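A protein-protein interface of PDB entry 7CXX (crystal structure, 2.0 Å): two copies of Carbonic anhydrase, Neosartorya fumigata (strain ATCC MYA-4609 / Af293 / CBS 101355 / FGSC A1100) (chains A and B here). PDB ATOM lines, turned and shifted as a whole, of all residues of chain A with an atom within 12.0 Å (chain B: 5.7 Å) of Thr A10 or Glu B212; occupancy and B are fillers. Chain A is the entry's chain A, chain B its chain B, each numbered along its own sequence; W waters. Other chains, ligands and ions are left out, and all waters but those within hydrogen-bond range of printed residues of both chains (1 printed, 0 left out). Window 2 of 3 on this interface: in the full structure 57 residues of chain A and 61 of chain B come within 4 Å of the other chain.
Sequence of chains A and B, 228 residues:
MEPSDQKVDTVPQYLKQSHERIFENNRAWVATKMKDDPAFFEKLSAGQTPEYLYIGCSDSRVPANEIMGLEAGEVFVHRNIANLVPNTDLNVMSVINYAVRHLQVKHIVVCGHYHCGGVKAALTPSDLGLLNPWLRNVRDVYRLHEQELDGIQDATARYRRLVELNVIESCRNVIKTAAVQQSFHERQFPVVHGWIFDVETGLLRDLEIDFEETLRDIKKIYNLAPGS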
ATOM      1  N   ASP A   9      15.201  -7.070 -16.963  1.00  0.00           N
ATOM      2  CA  ASP A   9      14.660  -7.261 -15.582  1.00  0.00           C
ATOM      3  C   ASP A   9      15.483  -8.321 -14.826  1.00  0.00           C
ATOM      4  O   ASP A   9      15.398  -8.340 -13.601  1.00  0.00           O
ATOM      5  CB  ASP A   9      13.174  -7.635 -15.630  1.00  0.00           C
ATOM      6  CG  ASP A   9      12.354  -7.093 -14.469  1.00  0.00           C
ATOM      7  OD1 ASP A   9      12.888  -7.035 -13.336  1.00  0.00           O
ATOM      8  OD2 ASP A   9      11.178  -6.735 -14.705  1.00  0.00           O
ATOM      9  N   THR A  10      16.232  -9.201 -15.503  1.00  0.00           N
ATOM     10  CA  THR A  10      17.199 -10.118 -14.828  1.00  0.00           C
ATOM     11  C   THR A  10      18.524  -9.366 -14.593  1.00  0.00           C
ATOM     12  O   THR A  10      18.794  -8.367 -15.285  1.00  0.00           O
ATOM     13  CB  THR A  10      17.422 -11.435 -15.587  1.00  0.00           C
ATOM     14  OG1 THR A  10      18.143 -11.158 -16.784  1.00  0.00           O
ATOM     15  CG2 THR A  10      16.145 -12.163 -15.940  1.00  0.00           C
ATOM     16  N   VAL A  11      19.288  -9.811 -13.604  1.00  0.00           N
ATOM     17  CA  VAL A  11      20.644  -9.287 -13.272  1.00  0.00           C
ATOM     18  C   VAL A  11      21.593  -9.763 -14.371  1.00  0.00           C
ATOM     19  O   VAL A  11      21.772 -10.965 -14.547  1.00  0.00           O
ATOM     20  CB  VAL A  11      21.087  -9.804 -11.890  1.00  0.00           C
ATOM     21  CG1 VAL A  11      22.557  -9.547 -11.604  1.00  0.00           C
ATOM     22  CG2 VAL A  11      20.194  -9.288 -10.766  1.00  0.00           C
ATOM     23  N   PRO A  12      22.207  -8.859 -15.164  1.00  0.00           N
ATOM     24  CA  PRO A  12      23.292  -9.244 -16.066  1.00  0.00           C
ATOM     25  C   PRO A  12      24.252 -10.223 -15.386  1.00  0.00           C
ATOM     26  O   PRO A  12      24.457 -10.105 -14.216  1.00  0.00           O
ATOM     27  CB  PRO A  12      23.971  -7.897 -16.352  1.00  0.00           C
ATOM     28  CG  PRO A  12      22.837  -6.897 -16.312  1.00  0.00           C
ATOM     29  CD  PRO A  12      21.892  -7.424 -15.249  1.00  0.00           C
ATOM     30  N   GLN A  13      24.803 -11.185 -16.127  1.00  0.00           N
ATOM     31  CA  GLN A  13      25.737 -12.207 -15.581  1.00  0.00           C
ATOM     32  C   GLN A  13      27.056 -11.543 -15.161  1.00  0.00           C
ATOM     33  O   GLN A  13      27.692 -12.001 -14.185  1.00  0.00           O
ATOM     34  CB  GLN A  13      26.018 -13.293 -16.636  1.00  0.00           C
ATOM     35  CG  GLN A  13      26.789 -14.488 -16.076  1.00  0.00           C
ATOM     36  CD  GLN A  13      25.968 -15.328 -15.124  1.00  0.00           C
ATOM     37  OE1 GLN A  13      24.775 -15.557 -15.336  1.00  0.00           O
ATOM     38  NE2 GLN A  13      26.598 -15.791 -14.054  1.00  0.00           N
ATOM     39  N   TYR A  14      27.506 -10.517 -15.870  1.00  0.00           N
ATOM     40  CA  TYR A  14      28.813  -9.900 -15.519  1.00  0.00           C
ATOM     41  C   TYR A  14      28.737  -9.344 -14.097  1.00  0.00           C
ATOM     42  O   TYR A  14      29.756  -9.339 -13.427  1.00  0.00           O
ATOM     43  CB  TYR A  14      29.212  -8.831 -16.524  1.00  0.00           C
ATOM     44  CG  TYR A  14      28.578  -7.478 -16.299  1.00  0.00           C
ATOM     45  CD1 TYR A  14      27.328  -7.187 -16.803  1.00  0.00           C
ATOM     46  CD2 TYR A  14      29.233  -6.488 -15.579  1.00  0.00           C
ATOM     47  CE1 TYR A  14      26.747  -5.939 -16.625  1.00  0.00           C
ATOM     48  CE2 TYR A  14      28.655  -5.241 -15.381  1.00  0.00           C
ATOM     49  CZ  TYR A  14      27.412  -4.963 -15.905  1.00  0.00           C
ATOM     50  OH  TYR A  14      26.853  -3.723 -15.785  1.00  0.00           O
ATOM     51  N   LEU A  15      27.539  -8.975 -13.628  1.00  0.00           N
ATOM     52  CA  LEU A  15      27.344  -8.445 -12.249  1.00  0.00           C
ATOM     53  C   LEU A  15      27.411  -9.606 -11.259  1.00  0.00           C
ATOM     54  O   LEU A  15      28.060  -9.439 -10.214  1.00  0.00           O
ATOM     55  CB  LEU A  15      26.042  -7.612 -12.176  1.00  0.00           C
ATOM     56  CG  LEU A  15      26.050  -6.290 -12.959  1.00  0.00           C
ATOM     57  CD1 LEU A  15      24.687  -5.640 -13.033  1.00  0.00           C
ATOM     58  CD2 LEU A  15      27.047  -5.298 -12.395  1.00  0.00           C
ATOM     59  N   LYS A  16      26.853 -10.782 -11.602  1.00  0.00           N
ATOM     60  CA  LYS A  16      26.918 -12.004 -10.755  1.00  0.00           C
ATOM     61  C   LYS A  16      28.379 -12.472 -10.579  1.00  0.00           C
ATOM     62  O   LYS A  16      28.771 -12.833  -9.452  1.00  0.00           O
ATOM     63  CB  LYS A  16      26.037 -13.109 -11.353  1.00  0.00           C
ATOM     64  CG  LYS A  16      24.561 -12.746 -11.465  1.00  0.00           C
ATOM     65  CD  LYS A  16      23.600 -13.934 -11.448  1.00  0.00           C
ATOM     66  CE  LYS A  16      22.177 -13.525 -11.110  1.00  0.00           C
ATOM     67  NZ  LYS A  16      21.185 -14.130 -12.038  1.00  0.00           N
ATOM     68  N   GLN A  17      29.182 -12.459 -11.635  1.00  0.00           N
ATOM     69  CA  GLN A  17      30.583 -12.962 -11.538  1.00  0.00           C
ATOM     70  C   GLN A  17      31.463 -11.880 -10.895  1.00  0.00           C
ATOM     71  O   GLN A  17      32.303 -12.260 -10.064  1.00  0.00           O
ATOM     72  CB  GLN A  17      31.087 -13.519 -12.879  1.00  0.00           C
ATOM     73  CG  GLN A  17      30.989 -12.574 -14.066  1.00  0.00           C
ATOM     74  CD  GLN A  17      30.850 -13.319 -15.379  1.00  0.00           C
ATOM     75  OE1 GLN A  17      31.184 -14.500 -15.493  1.00  0.00           O
ATOM     76  NE2 GLN A  17      30.367 -12.628 -16.403  1.00  0.00           N
ATOM     77  N   HIS A  19      30.454 -10.088  -8.511  1.00  0.00           N
ATOM     78  CA  HIS A  19      30.092 -10.344  -7.091  1.00  0.00           C
ATOM     79  C   HIS A  19      30.831 -11.591  -6.591  1.00  0.00           C
ATOM     80  O   HIS A  19      31.378 -11.516  -5.482  1.00  0.00           O
ATOM     81  CB  HIS A  19      28.558 -10.406  -6.913  1.00  0.00           C
ATOM     82  CG  HIS A  19      28.130 -10.513  -5.487  1.00  0.00           C
ATOM     83  ND1 HIS A  19      27.207 -11.449  -5.056  1.00  0.00           N
ATOM     84  CD2 HIS A  19      28.523  -9.828  -4.386  1.00  0.00           C
ATOM     85  CE1 HIS A  19      27.047 -11.337  -3.753  1.00  0.00           C
ATOM     86  NE2 HIS A  19      27.845 -10.336  -3.314  1.00  0.00           N
ATOM     87  N   PHE B 184      18.059   0.537 -12.272  1.00  0.00           N
ATOM     88  CA  PHE B 184      18.009  -0.894 -12.636  1.00  0.00           C
ATOM     89  C   PHE B 184      17.058  -1.077 -13.827  1.00  0.00           C
ATOM     90  O   PHE B 184      17.455  -1.813 -14.737  1.00  0.00           O
ATOM     91  CB  PHE B 184      17.660  -1.805 -11.456  1.00  0.00           C
ATOM     92  CG  PHE B 184      17.894  -3.243 -11.825  1.00  0.00           C
ATOM     93  CD1 PHE B 184      19.182  -3.762 -11.832  1.00  0.00           C
ATOM     94  CD2 PHE B 184      16.858  -4.042 -12.290  1.00  0.00           C
ATOM     95  CE1 PHE B 184      19.428  -5.066 -12.221  1.00  0.00           C
ATOM     96  CE2 PHE B 184      17.099  -5.356 -12.655  1.00  0.00           C
ATOM     97  CZ  PHE B 184      18.385  -5.858 -12.639  1.00  0.00           C
ATOM     98  N   GLN B 188      19.920  -1.698 -16.019  1.00  0.00           N
ATOM     99  CA  GLN B 188      20.216  -3.040 -15.422  1.00  0.00           C
ATOM    100  C   GLN B 188      21.425  -3.012 -14.456  1.00  0.00           C
ATOM    101  O   GLN B 188      22.116  -4.049 -14.294  1.00  0.00           O
ATOM    102  CB  GLN B 188      20.389  -4.060 -16.558  1.00  0.00           C
ATOM    103  CG  GLN B 188      19.118  -4.280 -17.379  1.00  0.00           C
ATOM    104  CD  GLN B 188      18.810  -3.126 -18.302  1.00  0.00           C
ATOM    105  OE1 GLN B 188      19.673  -2.633 -19.042  1.00  0.00           O
ATOM    106  NE2 GLN B 188      17.562  -2.674 -18.259  1.00  0.00           N
ATOM    107  N   ASP B 210      16.672 -11.593  -2.102  1.00  0.00           N
ATOM    108  CA  ASP B 210      15.706 -11.715  -3.223  1.00  0.00           C
ATOM    109  C   ASP B 210      15.642 -10.393  -3.996  1.00  0.00           C
ATOM    110  O   ASP B 210      14.601  -9.723  -3.912  1.00  0.00           O
ATOM    111  CB  ASP B 210      14.334 -12.081  -2.646  1.00  0.00           C
ATOM    112  CG  ASP B 210      14.347 -13.297  -1.734  1.00  0.00           C
ATOM    113  OD1 ASP B 210      14.652 -14.380  -2.227  1.00  0.00           O
ATOM    114  OD2 ASP B 210      14.051 -13.149  -0.554  1.00  0.00           O
ATOM    115  N   PHE B 211      16.691 -10.057  -4.746  1.00  0.00           N
ATOM    116  CA  PHE B 211      16.732  -8.756  -5.461  1.00  0.00           C
ATOM    117  C   PHE B 211      15.634  -8.636  -6.517  1.00  0.00           C
ATOM    118  O   PHE B 211      14.867  -7.672  -6.488  1.00  0.00           O
ATOM    119  CB  PHE B 211      18.067  -8.595  -6.187  1.00  0.00           C
ATOM    120  CG  PHE B 211      18.229  -7.279  -6.896  1.00  0.00           C
ATOM    121  CD1 PHE B 211      18.529  -6.129  -6.191  1.00  0.00           C
ATOM    122  CD2 PHE B 211      18.073  -7.184  -8.260  1.00  0.00           C
ATOM    123  CE1 PHE B 211      18.674  -4.921  -6.841  1.00  0.00           C
ATOM    124  CE2 PHE B 211      18.216  -5.975  -8.907  1.00  0.00           C
ATOM    125  CZ  PHE B 211      18.512  -4.845  -8.195  1.00  0.00           C
ATOM    126  N   GLU B 212      15.507  -9.648  -7.365  1.00  0.00           N
ATOM    127  CA  GLU B 212      14.502  -9.623  -8.453  1.00  0.00           C
ATOM    128  C   GLU B 212      13.091  -9.606  -7.851  1.00  0.00           C
ATOM    129  O   GLU B 212      12.275  -8.808  -8.299  1.00  0.00           O
ATOM    130  CB  GLU B 212      14.777 -10.786  -9.406  1.00  0.00           C
ATOM    131  CG  GLU B 212      15.905 -10.519 -10.391  1.00  0.00           C
ATOM    132  CD  GLU B 212      16.421 -11.715 -11.178  1.00  0.00           C
ATOM    133  OE1 GLU B 212      15.681 -12.711 -11.323  1.00  0.00           O
ATOM    134  OE2 GLU B 212      17.574 -11.656 -11.639  1.00  0.00           O
ATOM    135  N   GLU B 213      12.858 -10.420  -6.825  1.00  0.00           N
ATOM    136  CA  GLU B 213      11.540 -10.558  -6.157  1.00  0.00           C
ATOM    137  C   GLU B 213      11.125  -9.263  -5.456  1.00  0.00           C
ATOM    138  O   GLU B 213       9.960  -8.866  -5.616  1.00  0.00           O
ATOM    139  CB  GLU B 213      11.607 -11.708  -5.161  1.00  0.00           C
ATOM    140  CG  GLU B 213      10.305 -11.951  -4.436  1.00  0.00           C
ATOM    141  CD  GLU B 213      10.455 -12.808  -3.195  1.00  0.00           C
ATOM    142  OE1 GLU B 213      10.713 -14.006  -3.350  1.00  0.00           O
ATOM    143  OE2 GLU B 213      10.336 -12.260  -2.076  1.00  0.00           O
ATOM    144  N   THR B 214      12.060  -8.614  -4.749  1.00  0.00           N
ATOM    145  CA  THR B 214      11.756  -7.341  -4.053  1.00  0.00           C
ATOM    146  C   THR B 214      11.383  -6.307  -5.104  1.00  0.00           C
ATOM    147  O   THR B 214      10.394  -5.594  -4.921  1.00  0.00           O
ATOM    148  CB  THR B 214      12.962  -6.812  -3.274  1.00  0.00           C
ATOM    149  OG1 THR B 214      13.305  -7.751  -2.263  1.00  0.00           O
ATOM    150  CG2 THR B 214      12.705  -5.465  -2.636  1.00  0.00           C
ATOM    151  N   LEU B 215      12.132  -6.287  -6.197  1.00  0.00           N
ATOM    152  CA  LEU B 215      11.835  -5.342  -7.280  1.00  0.00           C
ATOM    153  C   LEU B 215      10.433  -5.648  -7.823  1.00  0.00           C
ATOM    154  O   LEU B 215       9.670  -4.718  -8.008  1.00  0.00           O
ATOM    155  CB  LEU B 215      12.916  -5.542  -8.335  1.00  0.00           C
ATOM    156  CG  LEU B 215      13.428  -4.271  -8.990  1.00  0.00           C
ATOM    157  CD1 LEU B 215      13.914  -3.309  -7.943  1.00  0.00           C
ATOM    158  CD2 LEU B 215      14.546  -4.600  -9.943  1.00  0.00           C
ATOM    159  N   ARG B 216      10.092  -6.913  -8.038  1.00  0.00           N
ATOM    160  CA  ARG B 216       8.735  -7.245  -8.546  1.00  0.00           C
ATOM    161  C   ARG B 216       7.693  -6.888  -7.488  1.00  0.00           C
ATOM    162  O   ARG B 216       6.688  -6.307  -7.847  1.00  0.00           O
ATOM    163  CB  ARG B 216       8.673  -8.690  -9.038  1.00  0.00           C
ATOM    164  CG  ARG B 216       9.658  -8.947 -10.170  1.00  0.00           C
ATOM    165  CD  ARG B 216       9.480 -10.189 -11.014  1.00  0.00           C
ATOM    166  NE  ARG B 216      10.464 -11.203 -10.681  1.00  0.00           N
ATOM    167  CZ  ARG B 216      10.288 -12.086  -9.720  1.00  0.00           C
ATOM    168  NH1 ARG B 216       9.170 -12.075  -9.024  1.00  0.00           N
ATOM    169  NH2 ARG B 216      11.219 -12.981  -9.465  1.00  0.00           N
ATOM    170  N   ASP B 217       8.007  -7.154  -6.226  1.00  0.00           N
ATOM    171  CA  ASP B 217       7.095  -6.910  -5.081  1.00  0.00           C
ATOM    172  C   ASP B 217       6.764  -5.419  -5.008  1.00  0.00           C
ATOM    173  O   ASP B 217       5.594  -5.094  -4.866  1.00  0.00           O
ATOM    174  CB  ASP B 217       7.790  -7.347  -3.795  1.00  0.00           C
ATOM    175  CG  ASP B 217       6.916  -8.051  -2.781  1.00  0.00           C
ATOM    176  OD1 ASP B 217       5.738  -8.208  -3.043  1.00  0.00           O
ATOM    177  OD2 ASP B 217       7.436  -8.432  -1.732  1.00  0.00           O
HETATM  178  O   HOH W   1      24.350  -3.599 -16.768  1.00  0.00           O
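The side-chain carboxylate (OE2) of Glu B212 is in hydrogen-bond range of the backbone NH (N) of Val A11 (3.2 Å).
Hydrophobic or aromatic side chains of chain A within 4 Å of the printed part of chain B: Val A11, Pro A12 and Leu A15. Of the 10 printed residues of chain B, 4 touch a printed residue of chain A. Printed residues of chain B that touch a printed residue of chain A: Phe B184, Gln B188, Phe B211 and Glu B212. Hydrophobic or aromatic side chains of chain B within 4 Å of the printed part of chain A: Phe B184 and Phe B211. Among the printed residues, 8 pairs touch across the chains. Among the printed residues, no Asp or Glu carboxylate lies within 4 Å of a Lys or Arg side-chain nitrogen of the other chain.
Phe B184 touches Asp A9. O of Asp A9 touches CG of Glu B212 (3.9 Å). Thr A10 touches Phe B184 (O to CZ, 3.7 Å). Glu B212 touches Thr A10. CG2 of Val A11 touches CD2 of Phe B211, 3.9 Å away. Pro A12 touches Gln B188 (CD to O, 3.5 Å). Gln B188 touches Leu A15.
Water W1 lies within hydrogen-bond range of the side-chain hydroxyl (OH) of Tyr A14 (2.7 Å) and the backbone carbonyl oxygen (O) of Gln B188 (3.4 Å).
Thr A10 touches just these residues of chain B: Phe B184 (3.7 Å) and Glu B212 (3.6 Å). Glu B212 touches just these residues of chain A: Asp A9 (3.9 Å), Thr A10 (3.6 Å) and Val A11 (3.2 Å). Of chain A, only Pro A12 (3.5 Å) and Leu A15 (3.3 Å) come within 4 Å of Gln B188. Asp B210 touches none of the printed residues of chain A. No residue of chain A comes within 4 Å of Glu B213. Thr B214 touches none of the printed residues of chain A. No residue of chain A comes within 4 Å of Arg B216. Printed residues of chain B within 4 Å of Leu A15: Gln B188 (3.3 Å). Of the printed residues of chain B, Asp A9 touches Phe B184 (3.6 Å) and Glu B212 (3.9 Å). Printed residues of chain B within 4 Å of Val A11: Phe B211 and Glu B212. Printed residues of chain A within 4 Å of Phe B184: Asp A9 and Thr A10. His A19 touches none of the printed residues of chain B. Asp B217 touches none of the printed residues of chain A. The nearest residue of chain A that does not touch Glu B212 is Lys A16 (4.4 Å).
No position is printed for both chains. Of the 8 pairs that touch across the chains among the printed residues, none has its exchanged pair printed and touching as well.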
